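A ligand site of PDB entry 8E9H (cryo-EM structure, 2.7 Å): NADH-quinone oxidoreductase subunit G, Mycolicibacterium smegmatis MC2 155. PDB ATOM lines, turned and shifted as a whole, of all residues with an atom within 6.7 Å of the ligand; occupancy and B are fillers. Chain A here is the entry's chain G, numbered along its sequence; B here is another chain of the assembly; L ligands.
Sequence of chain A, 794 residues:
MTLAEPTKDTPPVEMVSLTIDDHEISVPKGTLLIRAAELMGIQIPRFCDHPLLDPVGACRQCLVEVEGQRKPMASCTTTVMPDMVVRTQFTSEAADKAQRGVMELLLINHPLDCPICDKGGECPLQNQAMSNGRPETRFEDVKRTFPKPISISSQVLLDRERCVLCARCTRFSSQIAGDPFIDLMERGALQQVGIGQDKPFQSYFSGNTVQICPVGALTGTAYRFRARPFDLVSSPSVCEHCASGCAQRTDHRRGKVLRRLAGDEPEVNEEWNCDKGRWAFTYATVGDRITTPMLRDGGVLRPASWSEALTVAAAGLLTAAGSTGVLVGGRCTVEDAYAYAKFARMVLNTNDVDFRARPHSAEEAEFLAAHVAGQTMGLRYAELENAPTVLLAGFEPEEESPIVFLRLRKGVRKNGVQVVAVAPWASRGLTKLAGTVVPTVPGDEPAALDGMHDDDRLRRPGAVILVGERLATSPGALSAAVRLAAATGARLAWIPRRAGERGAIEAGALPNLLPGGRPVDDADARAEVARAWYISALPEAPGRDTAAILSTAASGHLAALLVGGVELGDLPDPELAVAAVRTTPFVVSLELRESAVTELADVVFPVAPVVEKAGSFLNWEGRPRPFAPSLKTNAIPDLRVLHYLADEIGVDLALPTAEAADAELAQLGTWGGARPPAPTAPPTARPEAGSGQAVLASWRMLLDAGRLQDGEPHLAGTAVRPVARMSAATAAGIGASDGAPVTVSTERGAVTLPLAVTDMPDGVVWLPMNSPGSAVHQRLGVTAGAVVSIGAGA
A ring nitrogen (ND1) of His 110 sits close to the backbone carbonyl oxygen (O) of Arg 162 (3.4 Å). The side-chain sulfur (SG) of Cys 114 lies close to the side-chain amide nitrogen (NE2) of Gln 126 (3.2 Å). The backbone carbonyl oxygen (O) of Cys 114 is in hydrogen-bond range of the guanidinium group (NH2) of Arg 228 (3.3 Å). The backbone NH (N) of Lys 119 sits close to the side-chain sulfur (SG) of Cys 117 (3.3 Å). N of Gln 126 sits close to SG of Cys 123, 3.6 Å away. The guanidinium group (NH1) of Arg 162 is in hydrogen-bond range of the backbone carbonyl oxygen (O) of Gly 216 (3.3 Å). The guanidinium group (NH2) of Arg 162 is in salt-bridge range of the side-chain carboxylate (OD2) of Asp 113 (2.9 Å). The backbone NH of Gly 121 lies within hydrogen-bond range of the side-chain amide oxygen of Gln 126, 3.0 Å away.
NE2 of His 110 binds FE3 of the ligand (2.0 Å). The backbone NH (N) of Cys 114 sits close to a sulfur (S2) of the ligand, 3.1 Å away. An iron atom (FE1) of the ligand is bound by the side-chain sulfur (SG) of Cys 114, 2.2 Å away. An iron atom (FE4) of the ligand is bound by the side-chain sulfur of Cys 117 (2.3 Å). An iron atom (FE2) of the ligand is bound by the side-chain sulfur of Cys 123. The backbone NH (N) of Gly 216 lies close to a sulfur (S1) of the ligand, 3.2 Å away. A sulfur (S2) of the ligand sits close to the backbone NH (N) of Asp 113. N of Gly 120 sits close to S3 of the ligand (3.6 Å). The side-chain amide nitrogen of Gln 126 lies close to a sulfur (S3) of the ligand, at 3.6 Å.
Merely in contact with the ligand: Pro 111, Leu 125 and Val 215. Hydrophobic or aromatic side chains within 4 Å of the ligand: His 110, Leu 125 and Val 215. Of the 28 residues printed, 11 come within 4 Å of the ligand. The nearest printed residue that does not touch the ligand is Lys 119 (4.03 Å).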
ATOM      1  N   LEU A 107      -5.282 -19.123 -35.608  1.00  0.00           N
ATOM      2  CA  LEU A 107      -4.705 -17.861 -35.174  1.00  0.00           C
ATOM      3  C   LEU A 107      -3.876 -17.167 -36.236  1.00  0.00           C
ATOM      4  O   LEU A 107      -3.536 -15.992 -36.056  1.00  0.00           O
ATOM      5  CB  LEU A 107      -3.825 -18.092 -33.942  1.00  0.00           C
ATOM      6  CG  LEU A 107      -4.564 -18.323 -32.627  1.00  0.00           C
ATOM      7  CD1 LEU A 107      -3.568 -18.658 -31.526  1.00  0.00           C
ATOM      8  CD2 LEU A 107      -5.381 -17.114 -32.237  1.00  0.00           C
ATOM      9  N   HIS A 110      -5.759 -14.308 -37.605  1.00  0.00           N
ATOM     10  CA  HIS A 110      -6.434 -13.486 -36.612  1.00  0.00           C
ATOM     11  C   HIS A 110      -5.709 -12.161 -36.439  1.00  0.00           C
ATOM     12  O   HIS A 110      -4.477 -12.116 -36.502  1.00  0.00           O
ATOM     13  CB  HIS A 110      -6.507 -14.216 -35.288  1.00  0.00           C
ATOM     14  CG  HIS A 110      -7.695 -13.845 -34.457  1.00  0.00           C
ATOM     15  ND1 HIS A 110      -8.960 -14.319 -34.721  1.00  0.00           N
ATOM     16  CD2 HIS A 110      -7.805 -13.047 -33.368  1.00  0.00           C
ATOM     17  CE1 HIS A 110      -9.799 -13.827 -33.834  1.00  0.00           C
ATOM     18  NE2 HIS A 110      -9.121 -13.052 -33.006  1.00  0.00           N
ATOM     19  N   PRO A 111      -6.436 -11.058 -36.229  1.00  0.00           N
ATOM     20  CA  PRO A 111      -5.765  -9.774 -36.012  1.00  0.00           C
ATOM     21  C   PRO A 111      -5.124  -9.693 -34.644  1.00  0.00           C
ATOM     22  O   PRO A 111      -5.570 -10.329 -33.681  1.00  0.00           O
ATOM     23  CB  PRO A 111      -6.907  -8.757 -36.143  1.00  0.00           C
ATOM     24  CG  PRO A 111      -8.035  -9.502 -36.725  1.00  0.00           C
ATOM     25  CD  PRO A 111      -7.884 -10.894 -36.255  1.00  0.00           C
ATOM     26  N   LEU A 112      -4.081  -8.873 -34.556  1.00  0.00           N
ATOM     27  CA  LEU A 112      -3.433  -8.584 -33.275  1.00  0.00           C
ATOM     28  C   LEU A 112      -4.214  -7.498 -32.540  1.00  0.00           C
ATOM     29  O   LEU A 112      -3.721  -6.408 -32.253  1.00  0.00           O
ATOM     30  CB  LEU A 112      -1.989  -8.179 -33.508  1.00  0.00           C
ATOM     31  CG  LEU A 112      -1.009  -9.339 -33.658  1.00  0.00           C
ATOM     32  CD1 LEU A 112      -1.446 -10.267 -34.758  1.00  0.00           C
ATOM     33  CD2 LEU A 112       0.394  -8.826 -33.915  1.00  0.00           C
ATOM     34  N   ASP A 113      -5.474  -7.827 -32.230  1.00  0.00           N
ATOM     35  CA  ASP A 113      -6.429  -6.846 -31.744  1.00  0.00           C
ATOM     36  C   ASP A 113      -6.833  -7.035 -30.293  1.00  0.00           C
ATOM     37  O   ASP A 113      -7.702  -6.313 -29.810  1.00  0.00           O
ATOM     38  CB  ASP A 113      -7.699  -6.884 -32.611  1.00  0.00           C
ATOM     39  CG  ASP A 113      -7.550  -6.116 -33.890  1.00  0.00           C
ATOM     40  OD1 ASP A 113      -6.439  -5.648 -34.186  1.00  0.00           O
ATOM     41  OD2 ASP A 113      -8.556  -5.977 -34.612  1.00  0.00           O
ATOM     42  N   CYS A 114      -6.219  -7.969 -29.568  1.00  0.00           N
ATOM     43  CA  CYS A 114      -6.670  -8.257 -28.215  1.00  0.00           C
ATOM     44  C   CYS A 114      -6.750  -7.003 -27.349  1.00  0.00           C
ATOM     45  O   CYS A 114      -7.760  -6.840 -26.647  1.00  0.00           O
ATOM     46  CB  CYS A 114      -5.746  -9.285 -27.556  1.00  0.00           C
ATOM     47  SG  CYS A 114      -5.647 -10.857 -28.420  1.00  0.00           S
ATOM     48  N   PRO A 115      -5.772  -6.099 -27.355  1.00  0.00           N
ATOM     49  CA  PRO A 115      -5.922  -4.890 -26.545  1.00  0.00           C
ATOM     50  C   PRO A 115      -7.144  -4.073 -26.895  1.00  0.00           C
ATOM     51  O   PRO A 115      -7.781  -3.500 -25.991  1.00  0.00           O
ATOM     52  CB  PRO A 115      -4.623  -4.116 -26.848  1.00  0.00           C
ATOM     53  CG  PRO A 115      -3.666  -5.163 -27.255  1.00  0.00           C
ATOM     54  CD  PRO A 115      -4.473  -6.132 -28.037  1.00  0.00           C
ATOM     55  N   ILE A 116      -7.516  -4.006 -28.169  1.00  0.00           N
ATOM     56  CA  ILE A 116      -8.658  -3.202 -28.576  1.00  0.00           C
ATOM     57  C   ILE A 116      -9.927  -4.012 -28.807  1.00  0.00           C
ATOM     58  O   ILE A 116     -11.011  -3.435 -28.912  1.00  0.00           O
ATOM     59  CB  ILE A 116      -8.325  -2.400 -29.858  1.00  0.00           C
ATOM     60  CG1 ILE A 116      -8.020  -3.337 -31.015  1.00  0.00           C
ATOM     61  CG2 ILE A 116      -7.147  -1.496 -29.608  1.00  0.00           C
ATOM     62  CD1 ILE A 116      -8.232  -2.709 -32.360  1.00  0.00           C
ATOM     63  N   CYS A 117      -9.816  -5.328 -28.894  1.00  0.00           N
ATOM     64  CA  CYS A 117     -10.991  -6.161 -29.083  1.00  0.00           C
ATOM     65  C   CYS A 117     -11.907  -6.068 -27.867  1.00  0.00           C
ATOM     66  O   CYS A 117     -11.440  -6.142 -26.731  1.00  0.00           O
ATOM     67  CB  CYS A 117     -10.585  -7.611 -29.336  1.00  0.00           C
ATOM     68  SG  CYS A 117     -11.953  -8.727 -29.536  1.00  0.00           S
ATOM     69  N   ASP A 118     -13.202  -5.913 -28.106  1.00  0.00           N
ATOM     70  CA  ASP A 118     -14.151  -5.885 -26.999  1.00  0.00           C
ATOM     71  C   ASP A 118     -14.200  -7.217 -26.262  1.00  0.00           C
ATOM     72  O   ASP A 118     -14.402  -7.244 -25.053  1.00  0.00           O
ATOM     73  CB  ASP A 118     -15.548  -5.524 -27.507  1.00  0.00           C
ATOM     74  CG  ASP A 118     -15.732  -4.044 -27.681  1.00  0.00           C
ATOM     75  OD1 ASP A 118     -15.225  -3.268 -26.841  1.00  0.00           O
ATOM     76  OD2 ASP A 118     -16.390  -3.638 -28.665  1.00  0.00           O
ATOM     77  N   LYS A 119     -14.024  -8.316 -26.981  1.00  0.00           N
ATOM     78  CA  LYS A 119     -14.094  -9.629 -26.372  1.00  0.00           C
ATOM     79  C   LYS A 119     -12.875  -9.934 -25.509  1.00  0.00           C
ATOM     80  O   LYS A 119     -12.886 -10.943 -24.798  1.00  0.00           O
ATOM     81  CB  LYS A 119     -14.250 -10.690 -27.457  1.00  0.00           C
ATOM     82  CG  LYS A 119     -14.673 -12.051 -26.932  1.00  0.00           C
ATOM     83  CD  LYS A 119     -16.146 -12.115 -26.600  1.00  0.00           C
ATOM     84  CE  LYS A 119     -16.999 -12.283 -27.832  1.00  0.00           C
ATOM     85  NZ  LYS A 119     -18.401 -12.617 -27.491  1.00  0.00           N
ATOM     86  N   GLY A 120     -11.847  -9.103 -25.550  1.00  0.00           N
ATOM     87  CA  GLY A 120     -10.642  -9.362 -24.775  1.00  0.00           C
ATOM     88  C   GLY A 120     -10.922  -9.586 -23.314  1.00  0.00           C
ATOM     89  O   GLY A 120     -11.726  -8.875 -22.715  1.00  0.00           O
ATOM     90  N   GLY A 121     -10.274 -10.596 -22.733  1.00  0.00           N
ATOM     91  CA  GLY A 121     -10.500 -10.972 -21.360  1.00  0.00           C
ATOM     92  C   GLY A 121     -11.635 -11.952 -21.174  1.00  0.00           C
ATOM     93  O   GLY A 121     -11.645 -12.697 -20.196  1.00  0.00           O
ATOM     94  N   GLU A 122     -12.587 -11.956 -22.094  1.00  0.00           N
ATOM     95  CA  GLU A 122     -13.710 -12.879 -22.078  1.00  0.00           C
ATOM     96  C   GLU A 122     -13.806 -13.633 -23.401  1.00  0.00           C
ATOM     97  O   GLU A 122     -14.875 -14.066 -23.810  1.00  0.00           O
ATOM     98  CB  GLU A 122     -15.010 -12.139 -21.802  1.00  0.00           C
ATOM     99  CG  GLU A 122     -15.296 -11.014 -22.779  1.00  0.00           C
ATOM    100  CD  GLU A 122     -16.635 -10.361 -22.542  1.00  0.00           C
ATOM    101  OE1 GLU A 122     -16.983 -10.120 -21.377  1.00  0.00           O
ATOM    102  OE2 GLU A 122     -17.335 -10.070 -23.536  1.00  0.00           O
ATOM    103  N   CYS A 123     -12.672 -13.796 -24.073  1.00  0.00           N
ATOM    104  CA  CYS A 123     -12.641 -14.348 -25.412  1.00  0.00           C
ATOM    105  C   CYS A 123     -12.383 -15.841 -25.353  1.00  0.00           C
ATOM    106  O   CYS A 123     -11.319 -16.253 -24.862  1.00  0.00           O
ATOM    107  CB  CYS A 123     -11.572 -13.660 -26.251  1.00  0.00           C
ATOM    108  SG  CYS A 123     -11.467 -14.244 -27.937  1.00  0.00           S
ATOM    109  N   PRO A 124     -13.303 -16.693 -25.813  1.00  0.00           N
ATOM    110  CA  PRO A 124     -12.986 -18.122 -25.878  1.00  0.00           C
ATOM    111  C   PRO A 124     -11.748 -18.409 -26.701  1.00  0.00           C
ATOM    112  O   PRO A 124     -11.034 -19.363 -26.395  1.00  0.00           O
ATOM    113  CB  PRO A 124     -14.245 -18.723 -26.507  1.00  0.00           C
ATOM    114  CG  PRO A 124     -15.319 -17.822 -26.084  1.00  0.00           C
ATOM    115  CD  PRO A 124     -14.738 -16.443 -26.029  1.00  0.00           C
ATOM    116  N   LEU A 125     -11.485 -17.627 -27.748  1.00  0.00           N
ATOM    117  CA  LEU A 125     -10.273 -17.874 -28.528  1.00  0.00           C
ATOM    118  C   LEU A 125      -9.026 -17.653 -27.696  1.00  0.00           C
ATOM    119  O   LEU A 125      -8.094 -18.462 -27.745  1.00  0.00           O
ATOM    120  CB  LEU A 125     -10.249 -16.999 -29.775  1.00  0.00           C
ATOM    121  CG  LEU A 125      -9.021 -17.191 -30.656  1.00  0.00           C
ATOM    122  CD1 LEU A 125      -8.839 -18.630 -31.042  1.00  0.00           C
ATOM    123  CD2 LEU A 125      -9.134 -16.329 -31.893  1.00  0.00           C
ATOM    124  N   GLN A 126      -8.977 -16.571 -26.914  1.00  0.00           N
ATOM    125  CA  GLN A 126      -7.820 -16.342 -26.065  1.00  0.00           C
ATOM    126  C   GLN A 126      -7.623 -17.481 -25.081  1.00  0.00           C
ATOM    127  O   GLN A 126      -6.526 -18.039 -24.947  1.00  0.00           O
ATOM    128  CB  GLN A 126      -7.964 -15.027 -25.303  1.00  0.00           C
ATOM    129  CG  GLN A 126      -7.701 -13.795 -26.119  1.00  0.00           C
ATOM    130  CD  GLN A 126      -7.719 -12.544 -25.278  1.00  0.00           C
ATOM    131  OE1 GLN A 126      -8.565 -12.388 -24.408  1.00  0.00           O
ATOM    132  NE2 GLN A 126      -6.779 -11.660 -25.532  1.00  0.00           N
ATOM    133  N   ARG A 162     -11.544 -10.887 -37.238  1.00  0.00           N
ATOM    134  CA  ARG A 162     -11.544 -11.715 -36.052  1.00  0.00           C
ATOM    135  C   ARG A 162     -12.430 -12.949 -36.192  1.00  0.00           C
ATOM    136  O   ARG A 162     -12.307 -13.880 -35.399  1.00  0.00           O
ATOM    137  CB  ARG A 162     -12.010 -10.909 -34.846  1.00  0.00           C
ATOM    138  CG  ARG A 162     -11.098  -9.760 -34.479  1.00  0.00           C
ATOM    139  CD  ARG A 162     -11.730  -8.874 -33.439  1.00  0.00           C
ATOM    140  NE  ARG A 162     -11.018  -7.604 -33.315  1.00  0.00           N
ATOM    141  CZ  ARG A 162     -11.589  -6.464 -32.946  1.00  0.00           C
ATOM    142  NH1 ARG A 162     -12.877  -6.394 -32.655  1.00  0.00           N
ATOM    143  NH2 ARG A 162     -10.846  -5.364 -32.879  1.00  0.00           N
ATOM    144  N   PRO A 214     -17.813 -16.670 -30.453  1.00  0.00           N
ATOM    145  CA  PRO A 214     -16.675 -16.983 -29.594  1.00  0.00           C
ATOM    146  C   PRO A 214     -15.494 -16.047 -29.734  1.00  0.00           C
ATOM    147  O   PRO A 214     -14.443 -16.315 -29.158  1.00  0.00           O
ATOM    148  CB  PRO A 214     -16.308 -18.396 -30.054  1.00  0.00           C
ATOM    149  CG  PRO A 214     -16.645 -18.391 -31.482  1.00  0.00           C
ATOM    150  CD  PRO A 214     -17.903 -17.606 -31.590  1.00  0.00           C
ATOM    151  N   VAL A 215     -15.626 -14.964 -30.493  1.00  0.00           N
ATOM    152  CA  VAL A 215     -14.553 -14.003 -30.695  1.00  0.00           C
ATOM    153  C   VAL A 215     -15.165 -12.623 -30.799  1.00  0.00           C
ATOM    154  O   VAL A 215     -16.381 -12.448 -30.722  1.00  0.00           O
ATOM    155  CB  VAL A 215     -13.714 -14.319 -31.950  1.00  0.00           C
ATOM    156  CG1 VAL A 215     -12.926 -15.593 -31.747  1.00  0.00           C
ATOM    157  CG2 VAL A 215     -14.607 -14.431 -33.158  1.00  0.00           C
ATOM    158  N   GLY A 216     -14.315 -11.624 -30.983  1.00  0.00           N
ATOM    159  CA  GLY A 216     -14.792 -10.259 -31.077  1.00  0.00           C
ATOM    160  C   GLY A 216     -15.258  -9.882 -32.468  1.00  0.00           C
ATOM    161  O   GLY A 216     -15.186  -8.708 -32.850  1.00  0.00           O
ATOM    162  N   ALA A 217     -15.727 -10.858 -33.236  1.00  0.00           N
ATOM    163  CA  ALA A 217     -16.219 -10.577 -34.576  1.00  0.00           C
ATOM    164  C   ALA A 217     -17.516  -9.772 -34.490  1.00  0.00           C
ATOM    165  O   ALA A 217     -17.576  -8.646 -34.983  1.00  0.00           O
ATOM    166  CB  ALA A 217     -16.453 -11.865 -35.349  1.00  0.00           C
ATOM    167  N   ARG A 228     -13.900  -3.494 -19.885  1.00  0.00           N
ATOM    168  CA  ARG A 228     -13.359  -4.840 -19.925  1.00  0.00           C
ATOM    169  C   ARG A 228     -13.971  -5.679 -18.823  1.00  0.00           C
ATOM    170  O   ARG A 228     -14.554  -5.144 -17.874  1.00  0.00           O
ATOM    171  CB  ARG A 228     -11.833  -4.825 -19.761  1.00  0.00           C
ATOM    172  CG  ARG A 228     -11.101  -3.765 -20.556  1.00  0.00           C
ATOM    173  CD  ARG A 228     -11.534  -3.680 -22.006  1.00  0.00           C
ATOM    174  NE  ARG A 228     -11.198  -4.869 -22.780  1.00  0.00           N
ATOM    175  CZ  ARG A 228     -10.151  -4.974 -23.584  1.00  0.00           C
ATOM    176  NH1 ARG A 228      -9.257  -4.011 -23.682  1.00  0.00           N
ATOM    177  NH2 ARG A 228      -9.998  -6.076 -24.312  1.00  0.00           N
ATOM    178  N   MET B 354       0.522 -13.330 -32.978  1.00  0.00           N
ATOM    179  CA  MET B 354      -0.810 -13.398 -32.406  1.00  0.00           C
ATOM    180  C   MET B 354      -0.801 -14.214 -31.121  1.00  0.00           C
ATOM    181  O   MET B 354      -1.408 -13.813 -30.112  1.00  0.00           O
ATOM    182  CB  MET B 354      -1.777 -14.009 -33.419  1.00  0.00           C
ATOM    183  CG  MET B 354      -3.195 -14.205 -32.923  1.00  0.00           C
ATOM    184  SD  MET B 354      -4.103 -12.655 -32.861  1.00  0.00           S
ATOM    185  CE  MET B 354      -4.291 -12.431 -31.106  1.00  0.00           C
ATOM    186  N   LEU B 357       0.733 -12.122 -28.464  1.00  0.00           N
ATOM    187  CA  LEU B 357      -0.219 -11.142 -27.949  1.00  0.00           C
ATOM    188  C   LEU B 357      -1.214 -11.786 -26.994  1.00  0.00           C
ATOM    189  O   LEU B 357      -1.519 -11.235 -25.935  1.00  0.00           O
ATOM    190  CB  LEU B 357      -0.955 -10.470 -29.102  1.00  0.00           C
ATOM    191  CG  LEU B 357      -1.968  -9.400 -28.720  1.00  0.00           C
ATOM    192  CD1 LEU B 357      -1.317  -8.312 -27.894  1.00  0.00           C
ATOM    193  CD2 LEU B 357      -2.598  -8.832 -29.964  1.00  0.00           C
ATOM    194  N   ILE B 358      -1.749 -12.962 -27.359  1.00  0.00           N
ATOM    195  CA  ILE B 358      -2.703 -13.620 -26.488  1.00  0.00           C
ATOM    196  C   ILE B 358      -2.054 -13.949 -25.150  1.00  0.00           C
ATOM    197  O   ILE B 358      -2.647 -13.751 -24.088  1.00  0.00           O
ATOM    198  CB  ILE B 358      -3.269 -14.881 -27.154  1.00  0.00           C
ATOM    199  CG1 ILE B 358      -4.235 -14.487 -28.275  1.00  0.00           C
ATOM    200  CG2 ILE B 358      -3.965 -15.749 -26.126  1.00  0.00           C
ATOM    201  CD1 ILE B 358      -4.756 -15.669 -29.074  1.00  0.00           C
ATOM    202  N   PHE B 361      -1.571 -10.764 -23.082  1.00  0.00           N
ATOM    203  CA  PHE B 361      -2.855 -10.302 -22.573  1.00  0.00           C
ATOM    204  C   PHE B 361      -3.306 -11.154 -21.393  1.00  0.00           C
ATOM    205  O   PHE B 361      -3.674 -10.635 -20.340  1.00  0.00           O
ATOM    206  CB  PHE B 361      -3.881 -10.342 -23.709  1.00  0.00           C
ATOM    207  CG  PHE B 361      -5.172  -9.662 -23.385  1.00  0.00           C
ATOM    208  CD1 PHE B 361      -6.044 -10.204 -22.457  1.00  0.00           C
ATOM    209  CD2 PHE B 361      -5.525  -8.500 -24.015  1.00  0.00           C
ATOM    210  CE1 PHE B 361      -7.234  -9.584 -22.172  1.00  0.00           C
ATOM    211  CE2 PHE B 361      -6.715  -7.879 -23.740  1.00  0.00           C
ATOM    212  CZ  PHE B 361      -7.573  -8.425 -22.803  1.00  0.00           C
HETATM  213 FE1  LIG L   1      -7.796 -11.173 -29.005  1.00  0.00          FE
HETATM  214 FE2  LIG L   1      -9.999 -12.776 -28.830  1.00  0.00          FE
HETATM  215 FE3  LIG L   1      -9.023 -12.044 -31.277  1.00  0.00          FE
HETATM  216 FE4  LIG L   1     -10.256 -10.201 -29.688  1.00  0.00          FE
HETATM  217  S1  LIG L   1     -11.200 -12.042 -30.629  1.00  0.00           S
HETATM  218  S2  LIG L   1      -8.312  -9.937 -30.844  1.00  0.00           S
HETATM  219  S3  LIG L   1      -9.587 -10.891 -27.627  1.00  0.00           S
HETATM  220  S4  LIG L   1      -7.983 -13.329 -29.719  1.00  0.00           S
